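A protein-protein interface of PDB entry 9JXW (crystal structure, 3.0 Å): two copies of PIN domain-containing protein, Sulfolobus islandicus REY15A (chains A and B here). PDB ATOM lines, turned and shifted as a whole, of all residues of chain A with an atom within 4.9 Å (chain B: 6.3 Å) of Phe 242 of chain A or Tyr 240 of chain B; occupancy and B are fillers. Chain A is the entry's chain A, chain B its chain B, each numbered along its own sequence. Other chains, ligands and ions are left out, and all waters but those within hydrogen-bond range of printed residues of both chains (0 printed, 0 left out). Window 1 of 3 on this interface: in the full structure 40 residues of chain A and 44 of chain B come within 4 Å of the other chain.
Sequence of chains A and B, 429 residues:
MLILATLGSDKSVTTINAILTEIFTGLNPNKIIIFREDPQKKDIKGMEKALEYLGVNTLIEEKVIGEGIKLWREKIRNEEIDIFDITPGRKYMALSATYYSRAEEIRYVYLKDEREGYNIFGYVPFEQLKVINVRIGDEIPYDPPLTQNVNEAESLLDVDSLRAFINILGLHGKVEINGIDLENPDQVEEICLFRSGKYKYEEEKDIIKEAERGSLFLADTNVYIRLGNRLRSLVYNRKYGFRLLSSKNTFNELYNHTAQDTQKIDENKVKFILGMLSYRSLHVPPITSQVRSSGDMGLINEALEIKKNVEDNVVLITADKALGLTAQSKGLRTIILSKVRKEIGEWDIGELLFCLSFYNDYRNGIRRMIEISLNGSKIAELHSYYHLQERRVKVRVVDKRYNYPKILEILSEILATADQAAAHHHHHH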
ATOM      1  N   LEU A 231       4.850  24.489 -17.659  1.00  0.00           N
ATOM      2  CA  LEU A 231       5.300  23.103 -17.665  1.00  0.00           C
ATOM      3  C   LEU A 231       5.233  22.506 -19.063  1.00  0.00           C
ATOM      4  O   LEU A 231       6.055  21.650 -19.411  1.00  0.00           O
ATOM      5  CB  LEU A 231       4.463  22.285 -16.680  1.00  0.00           C
ATOM      6  CG  LEU A 231       4.896  20.845 -16.401  1.00  0.00           C
ATOM      7  CD1 LEU A 231       6.375  20.786 -16.052  1.00  0.00           C
ATOM      8  CD2 LEU A 231       4.056  20.262 -15.279  1.00  0.00           C
ATOM      9  N   ARG A 232       4.272  22.947 -19.878  1.00  0.00           N
ATOM     10  CA  ARG A 232       4.203  22.483 -21.260  1.00  0.00           C
ATOM     11  C   ARG A 232       5.442  22.900 -22.040  1.00  0.00           C
ATOM     12  O   ARG A 232       6.021  22.093 -22.776  1.00  0.00           O
ATOM     13  CB  ARG A 232       2.929  22.999 -21.934  1.00  0.00           C
ATOM     14  CG  ARG A 232       2.767  22.584 -23.393  1.00  0.00           C
ATOM     15  CD  ARG A 232       1.300  22.608 -23.823  1.00  0.00           C
ATOM     16  NE  ARG A 232       0.506  23.538 -23.029  1.00  0.00           N
ATOM     17  CZ  ARG A 232      -0.807  23.451 -22.863  1.00  0.00           C
ATOM     18  NH1 ARG A 232      -1.510  22.477 -23.418  1.00  0.00           N
ATOM     19  NH2 ARG A 232      -1.428  24.358 -22.115  1.00  0.00           N
ATOM     20  N   VAL A 235       8.519  20.831 -20.920  1.00  0.00           N
ATOM     21  CA  VAL A 235       8.526  19.423 -21.305  1.00  0.00           C
ATOM     22  C   VAL A 235       8.559  19.258 -22.820  1.00  0.00           C
ATOM     23  O   VAL A 235       9.239  18.367 -23.337  1.00  0.00           O
ATOM     24  CB  VAL A 235       7.304  18.713 -20.687  1.00  0.00           C
ATOM     25  CG1 VAL A 235       7.184  17.292 -21.214  1.00  0.00           C
ATOM     26  CG2 VAL A 235       7.399  18.715 -19.169  1.00  0.00           C
ATOM     27  N   TYR A 236       7.837  20.106 -23.551  1.00  0.00           N
ATOM     28  CA  TYR A 236       7.703  19.932 -24.992  1.00  0.00           C
ATOM     29  C   TYR A 236       9.040  20.150 -25.693  1.00  0.00           C
ATOM     30  O   TYR A 236       9.757  21.113 -25.408  1.00  0.00           O
ATOM     31  CB  TYR A 236       6.653  20.893 -25.548  1.00  0.00           C
ATOM     32  CG  TYR A 236       6.309  20.661 -27.004  1.00  0.00           C
ATOM     33  CD1 TYR A 236       7.012  21.301 -28.017  1.00  0.00           C
ATOM     34  CD2 TYR A 236       5.274  19.808 -27.364  1.00  0.00           C
ATOM     35  CE1 TYR A 236       6.699  21.092 -29.347  1.00  0.00           C
ATOM     36  CE2 TYR A 236       4.953  19.593 -28.692  1.00  0.00           C
ATOM     37  CZ  TYR A 236       5.669  20.238 -29.678  1.00  0.00           C
ATOM     38  OH  TYR A 236       5.355  20.028 -31.001  1.00  0.00           O
ATOM     39  N   TYR A 240      10.715  14.851 -29.693  1.00  0.00           N
ATOM     40  CA  TYR A 240       9.927  13.867 -28.961  1.00  0.00           C
ATOM     41  C   TYR A 240       8.509  14.321 -28.645  1.00  0.00           C
ATOM     42  O   TYR A 240       7.608  13.478 -28.575  1.00  0.00           O
ATOM     43  CB  TYR A 240      10.631  13.491 -27.654  1.00  0.00           C
ATOM     44  CG  TYR A 240      12.019  12.929 -27.847  1.00  0.00           C
ATOM     45  CD1 TYR A 240      12.201  11.625 -28.293  1.00  0.00           C
ATOM     46  CD2 TYR A 240      13.146  13.694 -27.579  1.00  0.00           C
ATOM     47  CE1 TYR A 240      13.465  11.103 -28.471  1.00  0.00           C
ATOM     48  CE2 TYR A 240      14.415  13.178 -27.754  1.00  0.00           C
ATOM     49  CZ  TYR A 240      14.570  11.882 -28.200  1.00  0.00           C
ATOM     50  OH  TYR A 240      15.832  11.363 -28.376  1.00  0.00           O
ATOM     51  N   GLY A 241       8.285  15.616 -28.447  1.00  0.00           N
ATOM     52  CA  GLY A 241       6.948  16.098 -28.158  1.00  0.00           C
ATOM     53  C   GLY A 241       6.689  16.395 -26.695  1.00  0.00           C
ATOM     54  O   GLY A 241       7.610  16.720 -25.940  1.00  0.00           O
ATOM     55  N   PHE A 242       5.423  16.296 -26.293  1.00  0.00           N
ATOM     56  CA  PHE A 242       4.992  16.558 -24.922  1.00  0.00           C
ATOM     57  C   PHE A 242       4.894  15.216 -24.203  1.00  0.00           C
ATOM     58  O   PHE A 242       3.928  14.471 -24.384  1.00  0.00           O
ATOM     59  CB  PHE A 242       3.664  17.305 -24.916  1.00  0.00           C
ATOM     60  CG  PHE A 242       3.215  17.742 -23.550  1.00  0.00           C
ATOM     61  CD1 PHE A 242       3.942  18.677 -22.831  1.00  0.00           C
ATOM     62  CD2 PHE A 242       2.061  17.221 -22.989  1.00  0.00           C
ATOM     63  CE1 PHE A 242       3.525  19.080 -21.577  1.00  0.00           C
ATOM     64  CE2 PHE A 242       1.640  17.621 -21.737  1.00  0.00           C
ATOM     65  CZ  PHE A 242       2.372  18.552 -21.030  1.00  0.00           C
ATOM     66  N   ARG A 243       5.897  14.915 -23.382  1.00  0.00           N
ATOM     67  CA  ARG A 243       6.038  13.613 -22.743  1.00  0.00           C
ATOM     68  C   ARG A 243       5.725  13.673 -21.250  1.00  0.00           C
ATOM     69  O   ARG A 243       6.377  13.016 -20.438  1.00  0.00           O
ATOM     70  CB  ARG A 243       7.441  13.058 -22.966  1.00  0.00           C
ATOM     71  CG  ARG A 243       7.812  12.932 -24.431  1.00  0.00           C
ATOM     72  CD  ARG A 243       9.220  12.410 -24.601  1.00  0.00           C
ATOM     73  NE  ARG A 243       9.335  11.060 -24.069  1.00  0.00           N
ATOM     74  CZ  ARG A 243       8.978   9.970 -24.733  1.00  0.00           C
ATOM     75  NH1 ARG A 243       8.451  10.043 -25.945  1.00  0.00           N
ATOM     76  NH2 ARG A 243       9.130   8.780 -24.159  1.00  0.00           N
ATOM     77  N   LEU A 244       4.728  14.470 -20.873  1.00  0.00           N
ATOM     78  CA  LEU A 244       4.276  14.561 -19.487  1.00  0.00           C
ATOM     79  C   LEU A 244       3.052  13.669 -19.308  1.00  0.00           C
ATOM     80  O   LEU A 244       1.980  13.958 -19.849  1.00  0.00           O
ATOM     81  CB  LEU A 244       3.959  16.007 -19.112  1.00  0.00           C
ATOM     82  CG  LEU A 244       3.302  16.215 -17.745  1.00  0.00           C
ATOM     83  CD1 LEU A 244       4.188  15.690 -16.623  1.00  0.00           C
ATOM     84  CD2 LEU A 244       2.977  17.683 -17.528  1.00  0.00           C
ATOM     85  N   LEU A 282      -2.993  21.336 -19.302  1.00  0.00           N
ATOM     86  CA  LEU A 282      -1.747  20.735 -19.769  1.00  0.00           C
ATOM     87  C   LEU A 282      -1.992  19.390 -20.442  1.00  0.00           C
ATOM     88  O   LEU A 282      -1.690  19.209 -21.627  1.00  0.00           O
ATOM     89  CB  LEU A 282      -0.765  20.579 -18.605  1.00  0.00           C
ATOM     90  CG  LEU A 282      -0.079  21.846 -18.096  1.00  0.00           C
ATOM     91  CD1 LEU A 282       0.617  21.574 -16.773  1.00  0.00           C
ATOM     92  CD2 LEU A 282       0.900  22.373 -19.124  1.00  0.00           C
ATOM     93  N   HIS A 283      -2.529  18.429 -19.700  1.00  0.00           N
ATOM     94  CA  HIS A 283      -2.710  17.079 -20.221  1.00  0.00           C
ATOM     95  C   HIS A 283      -4.093  16.581 -19.814  1.00  0.00           C
ATOM     96  O   HIS A 283      -4.970  17.353 -19.414  1.00  0.00           O
ATOM     97  CB  HIS A 283      -1.589  16.134 -19.759  1.00  0.00           C
ATOM     98  CG  HIS A 283      -1.319  16.178 -18.290  1.00  0.00           C
ATOM     99  ND1 HIS A 283      -2.310  16.017 -17.347  1.00  0.00           N
ATOM    100  CD2 HIS A 283      -0.165  16.333 -17.600  1.00  0.00           C
ATOM    101  CE1 HIS A 283      -1.781  16.088 -16.139  1.00  0.00           C
ATOM    102  NE2 HIS A 283      -0.481  16.278 -16.265  1.00  0.00           N
ATOM    103  N   PRO A 285      -6.039  15.044 -22.301  1.00  0.00           N
ATOM    104  CA  PRO A 285      -6.967  15.408 -23.385  1.00  0.00           C
ATOM    105  C   PRO A 285      -8.011  14.333 -23.660  1.00  0.00           C
ATOM    106  O   PRO A 285      -9.181  14.670 -23.895  1.00  0.00           O
ATOM    107  CB  PRO A 285      -6.042  15.621 -24.592  1.00  0.00           C
ATOM    108  CG  PRO A 285      -4.730  15.954 -23.987  1.00  0.00           C
ATOM    109  CD  PRO A 285      -4.641  15.102 -22.775  1.00  0.00           C
ATOM    110  N   ALA B 211      -4.290   7.956 -32.018  1.00  0.00           N
ATOM    111  CA  ALA B 211      -3.226   8.951 -31.942  1.00  0.00           C
ATOM    112  C   ALA B 211      -3.792  10.366 -31.952  1.00  0.00           C
ATOM    113  O   ALA B 211      -3.255  11.263 -31.290  1.00  0.00           O
ATOM    114  CB  ALA B 211      -2.242   8.755 -33.095  1.00  0.00           C
ATOM    115  N   GLU B 212      -4.872  10.587 -32.705  1.00  0.00           N
ATOM    116  CA  GLU B 212      -5.510  11.900 -32.723  1.00  0.00           C
ATOM    117  C   GLU B 212      -6.168  12.225 -31.389  1.00  0.00           C
ATOM    118  O   GLU B 212      -6.252  13.401 -31.014  1.00  0.00           O
ATOM    119  CB  GLU B 212      -6.539  11.976 -33.849  1.00  0.00           C
ATOM    120  CG  GLU B 212      -5.940  11.893 -35.247  1.00  0.00           C
ATOM    121  CD  GLU B 212      -7.002  11.798 -36.323  1.00  0.00           C
ATOM    122  OE1 GLU B 212      -8.201  11.909 -35.987  1.00  0.00           O
ATOM    123  OE2 GLU B 212      -6.639  11.614 -37.504  1.00  0.00           O
ATOM    124  N   ARG B 213      -6.645  11.211 -30.668  1.00  0.00           N
ATOM    125  CA  ARG B 213      -7.251  11.423 -29.360  1.00  0.00           C
ATOM    126  C   ARG B 213      -6.223  11.599 -28.248  1.00  0.00           C
ATOM    127  O   ARG B 213      -6.608  11.921 -27.121  1.00  0.00           O
ATOM    128  CB  ARG B 213      -8.188  10.260 -29.023  1.00  0.00           C
ATOM    129  CG  ARG B 213      -9.411  10.175 -29.922  1.00  0.00           C
ATOM    130  CD  ARG B 213     -10.284   8.983 -29.571  1.00  0.00           C
ATOM    131  NE  ARG B 213     -11.474   8.920 -30.413  1.00  0.00           N
ATOM    132  CZ  ARG B 213     -12.393   7.966 -30.343  1.00  0.00           C
ATOM    133  NH1 ARG B 213     -12.286   6.967 -29.483  1.00  0.00           N
ATOM    134  NH2 ARG B 213     -13.442   8.014 -31.158  1.00  0.00           N
ATOM    135  N   GLY B 214      -4.938  11.396 -28.532  1.00  0.00           N
ATOM    136  CA  GLY B 214      -3.896  11.585 -27.539  1.00  0.00           C
ATOM    137  C   GLY B 214      -3.826  10.490 -26.494  1.00  0.00           C
ATOM    138  O   GLY B 214      -3.969  10.755 -25.297  1.00  0.00           O
ATOM    139  N   SER B 215      -3.596   9.256 -26.934  1.00  0.00           N
ATOM    140  CA  SER B 215      -3.592   8.095 -26.059  1.00  0.00           C
ATOM    141  C   SER B 215      -2.249   7.379 -26.133  1.00  0.00           C
ATOM    142  O   SER B 215      -1.600   7.349 -27.183  1.00  0.00           O
ATOM    143  CB  SER B 215      -4.733   7.134 -26.426  1.00  0.00           C
ATOM    144  OG  SER B 215      -4.707   6.810 -27.805  1.00  0.00           O
ATOM    145  N   ASN B 237       1.500  12.582 -34.047  1.00  0.00           N
ATOM    146  CA  ASN B 237       0.589  13.665 -34.383  1.00  0.00           C
ATOM    147  C   ASN B 237       1.168  14.966 -33.847  1.00  0.00           C
ATOM    148  O   ASN B 237       1.915  14.973 -32.866  1.00  0.00           O
ATOM    149  CB  ASN B 237      -0.812  13.433 -33.809  1.00  0.00           C
ATOM    150  CG  ASN B 237      -0.849  13.566 -32.305  1.00  0.00           C
ATOM    151  OD1 ASN B 237      -1.022  14.661 -31.775  1.00  0.00           O
ATOM    152  ND2 ASN B 237      -0.686  12.448 -31.607  1.00  0.00           N
ATOM    153  N   ARG B 238       0.811  16.072 -34.501  1.00  0.00           N
ATOM    154  CA  ARG B 238       1.409  17.361 -34.162  1.00  0.00           C
ATOM    155  C   ARG B 238       1.014  17.822 -32.765  1.00  0.00           C
ATOM    156  O   ARG B 238       1.848  18.356 -32.023  1.00  0.00           O
ATOM    157  CB  ARG B 238       1.011  18.405 -35.200  1.00  0.00           C
ATOM    158  CG  ARG B 238       1.441  18.035 -36.595  1.00  0.00           C
ATOM    159  CD  ARG B 238       1.025  19.079 -37.600  1.00  0.00           C
ATOM    160  NE  ARG B 238       1.557  18.759 -38.916  1.00  0.00           N
ATOM    161  CZ  ARG B 238       1.346  19.480 -40.006  1.00  0.00           C
ATOM    162  NH1 ARG B 238       0.607  20.577 -39.978  1.00  0.00           N
ATOM    163  NH2 ARG B 238       1.890  19.090 -41.153  1.00  0.00           N
ATOM    164  N   LYS B 239      -0.253  17.636 -32.392  1.00  0.00           N
ATOM    165  CA  LYS B 239      -0.731  18.155 -31.115  1.00  0.00           C
ATOM    166  C   LYS B 239      -0.051  17.460 -29.941  1.00  0.00           C
ATOM    167  O   LYS B 239       0.449  18.118 -29.022  1.00  0.00           O
ATOM    168  CB  LYS B 239      -2.248  17.997 -31.021  1.00  0.00           C
ATOM    169  CG  LYS B 239      -3.036  18.823 -32.024  1.00  0.00           C
ATOM    170  CD  LYS B 239      -4.533  18.660 -31.803  1.00  0.00           C
ATOM    171  CE  LYS B 239      -5.338  19.501 -32.779  1.00  0.00           C
ATOM    172  NZ  LYS B 239      -6.801  19.350 -32.551  1.00  0.00           N
ATOM    173  N   TYR B 240      -0.018  16.130 -29.957  1.00  0.00           N
ATOM    174  CA  TYR B 240       0.437  15.358 -28.808  1.00  0.00           C
ATOM    175  C   TYR B 240       1.857  14.828 -28.947  1.00  0.00           C
ATOM    176  O   TYR B 240       2.554  14.690 -27.936  1.00  0.00           O
ATOM    177  CB  TYR B 240      -0.521  14.191 -28.563  1.00  0.00           C
ATOM    178  CG  TYR B 240      -1.952  14.645 -28.399  1.00  0.00           C
ATOM    179  CD1 TYR B 240      -2.373  15.260 -27.233  1.00  0.00           C
ATOM    180  CD2 TYR B 240      -2.881  14.458 -29.414  1.00  0.00           C
ATOM    181  CE1 TYR B 240      -3.673  15.684 -27.086  1.00  0.00           C
ATOM    182  CE2 TYR B 240      -4.192  14.876 -29.273  1.00  0.00           C
ATOM    183  CZ  TYR B 240      -4.583  15.488 -28.104  1.00  0.00           C
ATOM    184  OH  TYR B 240      -5.885  15.910 -27.945  1.00  0.00           O
ATOM    185  N   GLY B 241       2.300  14.527 -30.163  1.00  0.00           N
ATOM    186  CA  GLY B 241       3.640  14.023 -30.379  1.00  0.00           C
ATOM    187  C   GLY B 241       3.680  12.523 -30.579  1.00  0.00           C
ATOM    188  O   GLY B 241       2.698  11.911 -31.015  1.00  0.00           O
ATOM    189  N   PHE B 242       4.816  11.918 -30.254  1.00  0.00           N
ATOM    190  CA  PHE B 242       5.006  10.478 -30.398  1.00  0.00           C
ATOM    191  C   PHE B 242       4.774   9.841 -29.031  1.00  0.00           C
ATOM    192  O   PHE B 242       5.645   9.877 -28.159  1.00  0.00           O
ATOM    193  CB  PHE B 242       6.395  10.170 -30.947  1.00  0.00           C
ATOM    194  CG  PHE B 242       6.608   8.724 -31.294  1.00  0.00           C
ATOM    195  CD1 PHE B 242       5.875   8.129 -32.307  1.00  0.00           C
ATOM    196  CD2 PHE B 242       7.552   7.965 -30.622  1.00  0.00           C
ATOM    197  CE1 PHE B 242       6.065   6.804 -32.634  1.00  0.00           C
ATOM    198  CE2 PHE B 242       7.754   6.638 -30.943  1.00  0.00           C
ATOM    199  CZ  PHE B 242       7.009   6.054 -31.952  1.00  0.00           C
ATOM    200  N   ARG B 243       3.590   9.257 -28.848  1.00  0.00           N
ATOM    201  CA  ARG B 243       3.148   8.722 -27.563  1.00  0.00           C
ATOM    202  C   ARG B 243       3.153   7.196 -27.559  1.00  0.00           C
ATOM    203  O   ARG B 243       2.266   6.555 -26.990  1.00  0.00           O
ATOM    204  CB  ARG B 243       1.762   9.251 -27.207  1.00  0.00           C
ATOM    205  CG  ARG B 243       1.696  10.762 -27.091  1.00  0.00           C
ATOM    206  CD  ARG B 243       0.279  11.259 -26.859  1.00  0.00           C
ATOM    207  NE  ARG B 243      -0.346  10.817 -25.618  1.00  0.00           N
ATOM    208  CZ  ARG B 243      -0.172  11.400 -24.439  1.00  0.00           C
ATOM    209  NH1 ARG B 243       0.655  12.421 -24.287  1.00  0.00           N
ATOM    210  NH2 ARG B 243      -0.876  10.973 -23.394  1.00  0.00           N
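The side-chain amide oxygen (OD1) of Asn 237 of chain B is in hydrogen-bond range of the backbone NH (N) of Tyr 240 of chain B.
Among the printed residues, merely in contact across the chains: Pro 285 of chain A with Tyr 240 of chain B (3.3 Å), Arg 243 of chain A with Phe 242 of chain B (3.6 Å), Tyr 240 of chain A with Phe 242 of chain B (3.6 Å), Phe 242 of chain A with Tyr 240 of chain B (3.7 Å) and Phe 242 of chain A with Arg 243 of chain B (3.9 Å).
Phe 242 of chain A touches just these residues of chain B: Tyr 240 (3.7 Å) and Arg 243 (3.9 Å). Of the printed residues of chain B, Tyr 240 of chain A touches Phe 242 (3.6 Å). Printed residues of chain B within 4 Å of Pro 285 of chain A: Tyr 240. Of the printed residues of chain A, Phe 242 of chain B touches Tyr 240 and Arg 243. Printed residues of chain B within 4 Å of Arg 243 of chain A: Phe 242. Of the printed residues of chain A, Arg 243 of chain B touches Phe 242 (3.9 Å). Arg 213 of chain B touches none of the printed residues of chain A.
Hydrophobic or aromatic side chains of chain B that line the printed part of chain A: Tyr 240. Of the 12 printed residues of chain A, 4 touch a printed residue of chain B. Hydrophobic or aromatic side chains of chain A within 4 Å of the printed part of chain B: Pro 285. Among the printed residues, 5 pairs touch across the chains. Among the printed residues, no Asp or Glu carboxylate lies within 4 Å of a Lys or Arg side-chain nitrogen of the other chain.
Tyr 240 of chain A touches Phe 242 of chain B, and with the chains exchanged Phe 242 of chain A touches Tyr 240 of chain B. Phe 242 of chain A touches Arg 243 of chain B, and with the chains exchanged Arg 243 of chain A touches Phe 242 of chain B. Positions printed for both chains: 240, 241, 242 and 243.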
